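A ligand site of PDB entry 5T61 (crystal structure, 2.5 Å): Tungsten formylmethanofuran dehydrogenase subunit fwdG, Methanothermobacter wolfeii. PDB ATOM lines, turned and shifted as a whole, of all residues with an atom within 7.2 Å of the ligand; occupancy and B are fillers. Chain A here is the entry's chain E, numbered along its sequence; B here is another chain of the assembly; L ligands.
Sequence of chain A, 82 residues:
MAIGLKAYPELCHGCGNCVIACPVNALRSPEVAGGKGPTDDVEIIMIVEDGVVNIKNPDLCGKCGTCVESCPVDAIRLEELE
A sulfur (S3) of the ligand lies close to the backbone NH (N) of Cys 15 (3.8 Å). FE2 of the ligand is bound by SG of Cys 15. An iron atom (FE3) of the ligand is bound by the side-chain sulfur of Cys 71, at 2.7 Å. SG of Cys 18 binds FE1 of the ligand (2.7 Å). FE4 of the ligand is bound by SG of Cys 12, at 2.7 Å. N of Gly 16 lies close to S3 of the ligand, 3.6 Å away. The backbone NH (N) of His 13 lies close to a sulfur (S1) of the ligand, at 3.7 Å.
The side-chain sulfur (SG) of Cys 15 sits close to the side-chain amide nitrogen (ND2) of Asn 17 (3.2 Å). N of Ala 75 sits close to SG of Cys 71 (3.1 Å). The side-chain sulfur (SG) of Cys 71 lies close to the backbone NH (N) of Val 73, at 3.2 Å. The side-chain sulfur (SG) of Cys 71 sits close to the backbone NH (N) of Asp 74, 2.9 Å away. The side-chain sulfur (SG) of Cys 12 lies close to the backbone NH (N) of Val 53, at 3.3 Å. A ring nitrogen (ND1) of His 13 is in hydrogen-bond range of the backbone carbonyl oxygen of Met 154 of chain B. The backbone NH (N) of Tyr 8 sits at hydrogen-bond distance from the backbone carbonyl oxygen (O) of Ala 75, 2.7 Å away. N of Gly 14 sits close to O of Gly 51 (3.4 Å).
Gly 14 touches the ligand. Val 53 touches the ligand. CB of Ala 75 touches S2 of the ligand, at 3.8 Å. Hydrophobic or aromatic side chains within 4 Å of the ligand: Val 53 and Ala 75. Nine residues have an atom within 4 Å of the ligand: Cys 12, His 13, Gly 14, Cys 15, Gly 16, Cys 18, Val 53, Cys 71 and Ala 75. Along chain A the residues within 4 Å of the ligand span positions 12 to 75.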
ATOM      1  N   TYR A   8      13.989  20.027 -23.893  1.00  0.00           N
ATOM      2  CA  TYR A   8      15.271  20.048 -24.585  1.00  0.00           C
ATOM      3  C   TYR A   8      15.031  19.635 -26.031  1.00  0.00           C
ATOM      4  O   TYR A   8      15.308  18.485 -26.420  1.00  0.00           O
ATOM      5  CB  TYR A   8      16.288  19.138 -23.923  1.00  0.00           C
ATOM      6  CG  TYR A   8      16.769  19.614 -22.571  1.00  0.00           C
ATOM      7  CD1 TYR A   8      15.943  19.561 -21.463  1.00  0.00           C
ATOM      8  CD2 TYR A   8      18.061  20.128 -22.406  1.00  0.00           C
ATOM      9  CE1 TYR A   8      16.372  19.992 -20.224  1.00  0.00           C
ATOM     10  CE2 TYR A   8      18.500  20.565 -21.174  1.00  0.00           C
ATOM     11  CZ  TYR A   8      17.647  20.501 -20.087  1.00  0.00           C
ATOM     12  OH  TYR A   8      18.070  20.935 -18.854  1.00  0.00           O
ATOM     13  N   PRO A   9      14.512  20.543 -26.865  1.00  0.00           N
ATOM     14  CA  PRO A   9      14.152  20.142 -28.240  1.00  0.00           C
ATOM     15  C   PRO A   9      15.316  19.631 -29.059  1.00  0.00           C
ATOM     16  O   PRO A   9      15.105  18.833 -29.979  1.00  0.00           O
ATOM     17  CB  PRO A   9      13.568  21.439 -28.836  1.00  0.00           C
ATOM     18  CG  PRO A   9      14.063  22.534 -27.960  1.00  0.00           C
ATOM     19  CD  PRO A   9      14.201  21.958 -26.595  1.00  0.00           C
ATOM     20  N   LEU A  11      17.470  17.519 -28.322  1.00  0.00           N
ATOM     21  CA  LEU A  11      17.600  16.091 -28.095  1.00  0.00           C
ATOM     22  C   LEU A  11      16.357  15.306 -28.508  1.00  0.00           C
ATOM     23  O   LEU A  11      16.389  14.069 -28.541  1.00  0.00           O
ATOM     24  CB  LEU A  11      17.876  15.818 -26.611  1.00  0.00           C
ATOM     25  CG  LEU A  11      19.071  16.553 -25.977  1.00  0.00           C
ATOM     26  CD1 LEU A  11      19.082  16.347 -24.465  1.00  0.00           C
ATOM     27  CD2 LEU A  11      20.382  16.111 -26.593  1.00  0.00           C
ATOM     28  N   CYS A  12      15.271  16.004 -28.840  1.00  0.00           N
ATOM     29  CA  CYS A  12      13.953  15.414 -29.039  1.00  0.00           C
ATOM     30  C   CYS A  12      13.826  14.709 -30.378  1.00  0.00           C
ATOM     31  O   CYS A  12      14.391  15.128 -31.389  1.00  0.00           O
ATOM     32  CB  CYS A  12      12.896  16.506 -28.949  1.00  0.00           C
ATOM     33  SG  CYS A  12      11.342  16.021 -29.666  1.00  0.00           S
ATOM     34  N   HIS A  13      13.039  13.618 -30.383  1.00  0.00           N
ATOM     35  CA  HIS A  13      12.730  12.857 -31.593  1.00  0.00           C
ATOM     36  C   HIS A  13      11.395  13.210 -32.212  1.00  0.00           C
ATOM     37  O   HIS A  13      11.124  12.786 -33.339  1.00  0.00           O
ATOM     38  CB  HIS A  13      12.723  11.350 -31.300  1.00  0.00           C
ATOM     39  CG  HIS A  13      14.078  10.782 -30.994  1.00  0.00           C
ATOM     40  ND1 HIS A  13      14.404   9.469 -31.267  1.00  0.00           N
ATOM     41  CD2 HIS A  13      15.172  11.329 -30.440  1.00  0.00           C
ATOM     42  CE1 HIS A  13      15.649   9.239 -30.898  1.00  0.00           C
ATOM     43  NE2 HIS A  13      16.138  10.349 -30.391  1.00  0.00           N
ATOM     44  N   GLY A  14      10.540  13.951 -31.498  1.00  0.00           N
ATOM     45  CA  GLY A  14       9.180  14.132 -31.964  1.00  0.00           C
ATOM     46  C   GLY A  14       8.307  12.908 -31.830  1.00  0.00           C
ATOM     47  O   GLY A  14       7.266  12.816 -32.496  1.00  0.00           O
ATOM     48  N   CYS A  15       8.703  11.935 -30.994  1.00  0.00           N
ATOM     49  CA  CYS A  15       8.037  10.633 -31.022  1.00  0.00           C
ATOM     50  C   CYS A  15       6.629  10.710 -30.431  1.00  0.00           C
ATOM     51  O   CYS A  15       5.782   9.890 -30.767  1.00  0.00           O
ATOM     52  CB  CYS A  15       8.845   9.590 -30.263  1.00  0.00           C
ATOM     53  SG  CYS A  15       8.408   9.430 -28.539  1.00  0.00           S
ATOM     54  N   GLY A  16       6.395  11.657 -29.527  1.00  0.00           N
ATOM     55  CA  GLY A  16       5.060  11.875 -29.004  1.00  0.00           C
ATOM     56  C   GLY A  16       4.684  11.091 -27.759  1.00  0.00           C
ATOM     57  O   GLY A  16       3.531  11.213 -27.311  1.00  0.00           O
ATOM     58  N   ASN A  17       5.591  10.296 -27.177  1.00  0.00           N
ATOM     59  CA  ASN A  17       5.212   9.488 -26.023  1.00  0.00           C
ATOM     60  C   ASN A  17       4.786  10.375 -24.855  1.00  0.00           C
ATOM     61  O   ASN A  17       3.811  10.059 -24.164  1.00  0.00           O
ATOM     62  CB  ASN A  17       6.352   8.571 -25.587  1.00  0.00           C
ATOM     63  CG  ASN A  17       6.749   7.568 -26.660  1.00  0.00           C
ATOM     64  OD1 ASN A  17       5.990   7.306 -27.591  1.00  0.00           O
ATOM     65  ND2 ASN A  17       7.947   7.011 -26.530  1.00  0.00           N
ATOM     66  N   CYS A  18       5.510  11.469 -24.610  1.00  0.00           N
ATOM     67  CA  CYS A  18       5.150  12.347 -23.506  1.00  0.00           C
ATOM     68  C   CYS A  18       3.779  12.969 -23.735  1.00  0.00           C
ATOM     69  O   CYS A  18       2.981  13.074 -22.801  1.00  0.00           O
ATOM     70  CB  CYS A  18       6.181  13.463 -23.348  1.00  0.00           C
ATOM     71  SG  CYS A  18       5.988  14.739 -24.603  1.00  0.00           S
ATOM     72  N   VAL A  19       3.509  13.411 -24.962  1.00  0.00           N
ATOM     73  CA  VAL A  19       2.221  14.025 -25.283  1.00  0.00           C
ATOM     74  C   VAL A  19       1.082  13.071 -24.957  1.00  0.00           C
ATOM     75  O   VAL A  19       0.087  13.455 -24.340  1.00  0.00           O
ATOM     76  CB  VAL A  19       2.180  14.455 -26.765  1.00  0.00           C
ATOM     77  CG1 VAL A  19       0.804  14.976 -27.126  1.00  0.00           C
ATOM     78  CG2 VAL A  19       3.242  15.512 -27.037  1.00  0.00           C
ATOM     79  N   MET A  46       1.752  20.343 -23.807  1.00  0.00           N
ATOM     80  CA  MET A  46       2.748  20.397 -24.860  1.00  0.00           C
ATOM     81  C   MET A  46       2.288  19.542 -26.039  1.00  0.00           C
ATOM     82  O   MET A  46       1.467  18.635 -25.885  1.00  0.00           O
ATOM     83  CB  MET A  46       4.128  19.954 -24.387  1.00  0.00           C
ATOM     84  CG  MET A  46       4.244  18.479 -24.068  1.00  0.00           C
ATOM     85  SD  MET A  46       3.399  18.050 -22.540  1.00  0.00           S
ATOM     86  CE  MET A  46       4.185  16.478 -22.164  1.00  0.00           C
ATOM     87  N   VAL A  48       3.949  18.075 -30.139  1.00  0.00           N
ATOM     88  CA  VAL A  48       5.058  18.003 -31.090  1.00  0.00           C
ATOM     89  C   VAL A  48       4.757  18.991 -32.203  1.00  0.00           C
ATOM     90  O   VAL A  48       3.712  18.924 -32.855  1.00  0.00           O
ATOM     91  CB  VAL A  48       5.227  16.579 -31.642  1.00  0.00           C
ATOM     92  CG1 VAL A  48       6.291  16.558 -32.714  1.00  0.00           C
ATOM     93  CG2 VAL A  48       5.577  15.613 -30.522  1.00  0.00           C
ATOM     94  N   GLY A  51       8.467  18.972 -35.550  1.00  0.00           N
ATOM     95  CA  GLY A  51       9.286  17.810 -35.326  1.00  0.00           C
ATOM     96  C   GLY A  51       9.798  17.592 -33.908  1.00  0.00           C
ATOM     97  O   GLY A  51      10.499  16.595 -33.680  1.00  0.00           O
ATOM     98  N   VAL A  52       9.492  18.484 -32.960  1.00  0.00           N
ATOM     99  CA  VAL A  52      10.028  18.386 -31.601  1.00  0.00           C
ATOM    100  C   VAL A  52       8.981  18.816 -30.582  1.00  0.00           C
ATOM    101  O   VAL A  52       7.958  19.430 -30.905  1.00  0.00           O
ATOM    102  CB  VAL A  52      11.322  19.228 -31.409  1.00  0.00           C
ATOM    103  CG1 VAL A  52      12.457  18.686 -32.256  1.00  0.00           C
ATOM    104  CG2 VAL A  52      11.073  20.699 -31.707  1.00  0.00           C
ATOM    105  N   VAL A  53       9.259  18.492 -29.316  1.00  0.00           N
ATOM    106  CA  VAL A  53       8.365  18.833 -28.218  1.00  0.00           C
ATOM    107  C   VAL A  53       8.313  20.336 -28.050  1.00  0.00           C
ATOM    108  O   VAL A  53       9.319  21.037 -28.200  1.00  0.00           O
ATOM    109  CB  VAL A  53       8.832  18.192 -26.909  1.00  0.00           C
ATOM    110  CG1 VAL A  53       7.727  18.243 -25.845  1.00  0.00           C
ATOM    111  CG2 VAL A  53       9.178  16.838 -27.187  1.00  0.00           C
ATOM    112  N   CYS A  67       5.487  12.001 -18.017  1.00  0.00           N
ATOM    113  CA  CYS A  67       6.159  12.241 -19.292  1.00  0.00           C
ATOM    114  C   CYS A  67       7.638  11.907 -19.205  1.00  0.00           C
ATOM    115  O   CYS A  67       8.202  11.305 -20.133  1.00  0.00           O
ATOM    116  CB  CYS A  67       5.994  13.691 -19.731  1.00  0.00           C
ATOM    117  SG  CYS A  67       7.097  14.806 -18.837  1.00  0.00           S
ATOM    118  N   VAL A  68       8.285  12.301 -18.107  1.00  0.00           N
ATOM    119  CA  VAL A  68       9.717  12.067 -17.951  1.00  0.00           C
ATOM    120  C   VAL A  68      10.035  10.587 -18.071  1.00  0.00           C
ATOM    121  O   VAL A  68      10.968  10.184 -18.765  1.00  0.00           O
ATOM    122  CB  VAL A  68      10.217  12.656 -16.603  1.00  0.00           C
ATOM    123  CG1 VAL A  68      11.627  12.172 -16.300  1.00  0.00           C
ATOM    124  CG2 VAL A  68      10.190  14.175 -16.634  1.00  0.00           C
ATOM    125  N   SER A  70       8.354   8.419 -19.706  1.00  0.00           N
ATOM    126  CA  SER A  70       8.032   7.947 -21.044  1.00  0.00           C
ATOM    127  C   SER A  70       9.072   8.333 -22.091  1.00  0.00           C
ATOM    128  O   SER A  70       9.054   7.750 -23.187  1.00  0.00           O
ATOM    129  CB  SER A  70       6.657   8.488 -21.455  1.00  0.00           C
ATOM    130  OG  SER A  70       6.756   9.853 -21.801  1.00  0.00           O
ATOM    131  N   CYS A  71       9.945   9.294 -21.794  1.00  0.00           N
ATOM    132  CA  CYS A  71      10.979   9.719 -22.735  1.00  0.00           C
ATOM    133  C   CYS A  71      12.261   8.940 -22.516  1.00  0.00           C
ATOM    134  O   CYS A  71      12.839   9.013 -21.424  1.00  0.00           O
ATOM    135  CB  CYS A  71      11.273  11.196 -22.569  1.00  0.00           C
ATOM    136  SG  CYS A  71      12.881  11.639 -23.266  1.00  0.00           S
ATOM    137  N   PRO A  72      12.745   8.196 -23.525  1.00  0.00           N
ATOM    138  CA  PRO A  72      14.012   7.467 -23.328  1.00  0.00           C
ATOM    139  C   PRO A  72      15.260   8.321 -23.496  1.00  0.00           C
ATOM    140  O   PRO A  72      16.330   7.898 -23.044  1.00  0.00           O
ATOM    141  CB  PRO A  72      13.948   6.377 -24.410  1.00  0.00           C
ATOM    142  CG  PRO A  72      13.038   6.919 -25.467  1.00  0.00           C
ATOM    143  CD  PRO A  72      12.195   8.026 -24.876  1.00  0.00           C
ATOM    144  N   VAL A  73      15.171   9.511 -24.092  1.00  0.00           N
ATOM    145  CA  VAL A  73      16.353  10.303 -24.421  1.00  0.00           C
ATOM    146  C   VAL A  73      16.426  11.580 -23.597  1.00  0.00           C
ATOM    147  O   VAL A  73      17.145  12.517 -23.957  1.00  0.00           O
ATOM    148  CB  VAL A  73      16.411  10.610 -25.928  1.00  0.00           C
ATOM    149  CG1 VAL A  73      16.545   9.327 -26.731  1.00  0.00           C
ATOM    150  CG2 VAL A  73      15.186  11.391 -26.353  1.00  0.00           C
ATOM    151  N   ASP A  74      15.695  11.648 -22.471  1.00  0.00           N
ATOM    152  CA  ASP A  74      15.763  12.765 -21.524  1.00  0.00           C
ATOM    153  C   ASP A  74      15.603  14.118 -22.215  1.00  0.00           C
ATOM    154  O   ASP A  74      16.325  15.071 -21.938  1.00  0.00           O
ATOM    155  CB  ASP A  74      17.064  12.730 -20.722  1.00  0.00           C
ATOM    156  CG  ASP A  74      17.216  11.461 -19.905  1.00  0.00           C
ATOM    157  OD1 ASP A  74      16.257  10.659 -19.867  1.00  0.00           O
ATOM    158  OD2 ASP A  74      18.295  11.281 -19.297  1.00  0.00           O
ATOM    159  N   ALA A  75      14.645  14.202 -23.140  1.00  0.00           N
ATOM    160  CA  ALA A  75      14.374  15.451 -23.842  1.00  0.00           C
ATOM    161  C   ALA A  75      13.319  16.316 -23.153  1.00  0.00           C
ATOM    162  O   ALA A  75      13.183  17.491 -23.500  1.00  0.00           O
ATOM    163  CB  ALA A  75      13.934  15.162 -25.283  1.00  0.00           C
ATOM    164  N   ILE A  76      12.585  15.766 -22.181  1.00  0.00           N
ATOM    165  CA  ILE A  76      11.640  16.518 -21.368  1.00  0.00           C
ATOM    166  C   ILE A  76      11.881  16.150 -19.917  1.00  0.00           C
ATOM    167  O   ILE A  76      12.081  14.978 -19.584  1.00  0.00           O
ATOM    168  CB  ILE A  76      10.176  16.253 -21.787  1.00  0.00           C
ATOM    169  CG1 ILE A  76       9.231  17.222 -21.072  1.00  0.00           C
ATOM    170  CG2 ILE A  76       9.769  14.806 -21.557  1.00  0.00           C
ATOM    171  CD1 ILE A  76       7.833  17.253 -21.647  1.00  0.00           C
ATOM    172  N   MET B 154      11.877   3.975 -31.895  1.00  0.00           N
ATOM    173  CA  MET B 154      12.142   5.340 -31.450  1.00  0.00           C
ATOM    174  C   MET B 154      13.027   6.085 -32.441  1.00  0.00           C
ATOM    175  O   MET B 154      12.930   7.315 -32.564  1.00  0.00           O
ATOM    176  CB  MET B 154      12.777   5.341 -30.031  1.00  0.00           C
ATOM    177  CG  MET B 154      11.816   4.753 -29.007  1.00  0.00           C
ATOM    178  SD  MET B 154      10.342   5.734 -28.694  1.00  0.00           S
ATOM    179  CE  MET B 154      11.039   7.347 -28.419  1.00  0.00           C
ATOM    180  N   PRO B 158       9.233   6.724 -35.243  1.00  0.00           N
ATOM    181  CA  PRO B 158       9.253   7.432 -33.945  1.00  0.00           C
ATOM    182  C   PRO B 158       7.909   7.517 -33.241  1.00  0.00           C
ATOM    183  O   PRO B 158       7.865   7.439 -32.008  1.00  0.00           O
ATOM    184  CB  PRO B 158       9.775   8.822 -34.329  1.00  0.00           C
ATOM    185  CG  PRO B 158      10.639   8.548 -35.514  1.00  0.00           C
ATOM    186  CD  PRO B 158       9.913   7.495 -36.291  1.00  0.00           C
HETATM  187 FE1  LIG L   1       8.228  13.686 -25.597  1.00  0.00          FE
HETATM  188 FE2  LIG L   1       9.450  11.615 -27.749  1.00  0.00          FE
HETATM  189 FE3  LIG L   1      11.228  12.465 -25.183  1.00  0.00          FE
HETATM  190 FE4  LIG L   1      10.657  14.544 -27.553  1.00  0.00          FE
HETATM  191  S1  LIG L   1      11.241  12.579 -27.272  1.00  0.00           S
HETATM  192  S2  LIG L   1      10.241  14.262 -25.514  1.00  0.00           S
HETATM  193  S3  LIG L   1       8.800  13.578 -27.605  1.00  0.00           S
HETATM  194  S4  LIG L   1       9.283  11.879 -25.683  1.00  0.00           S
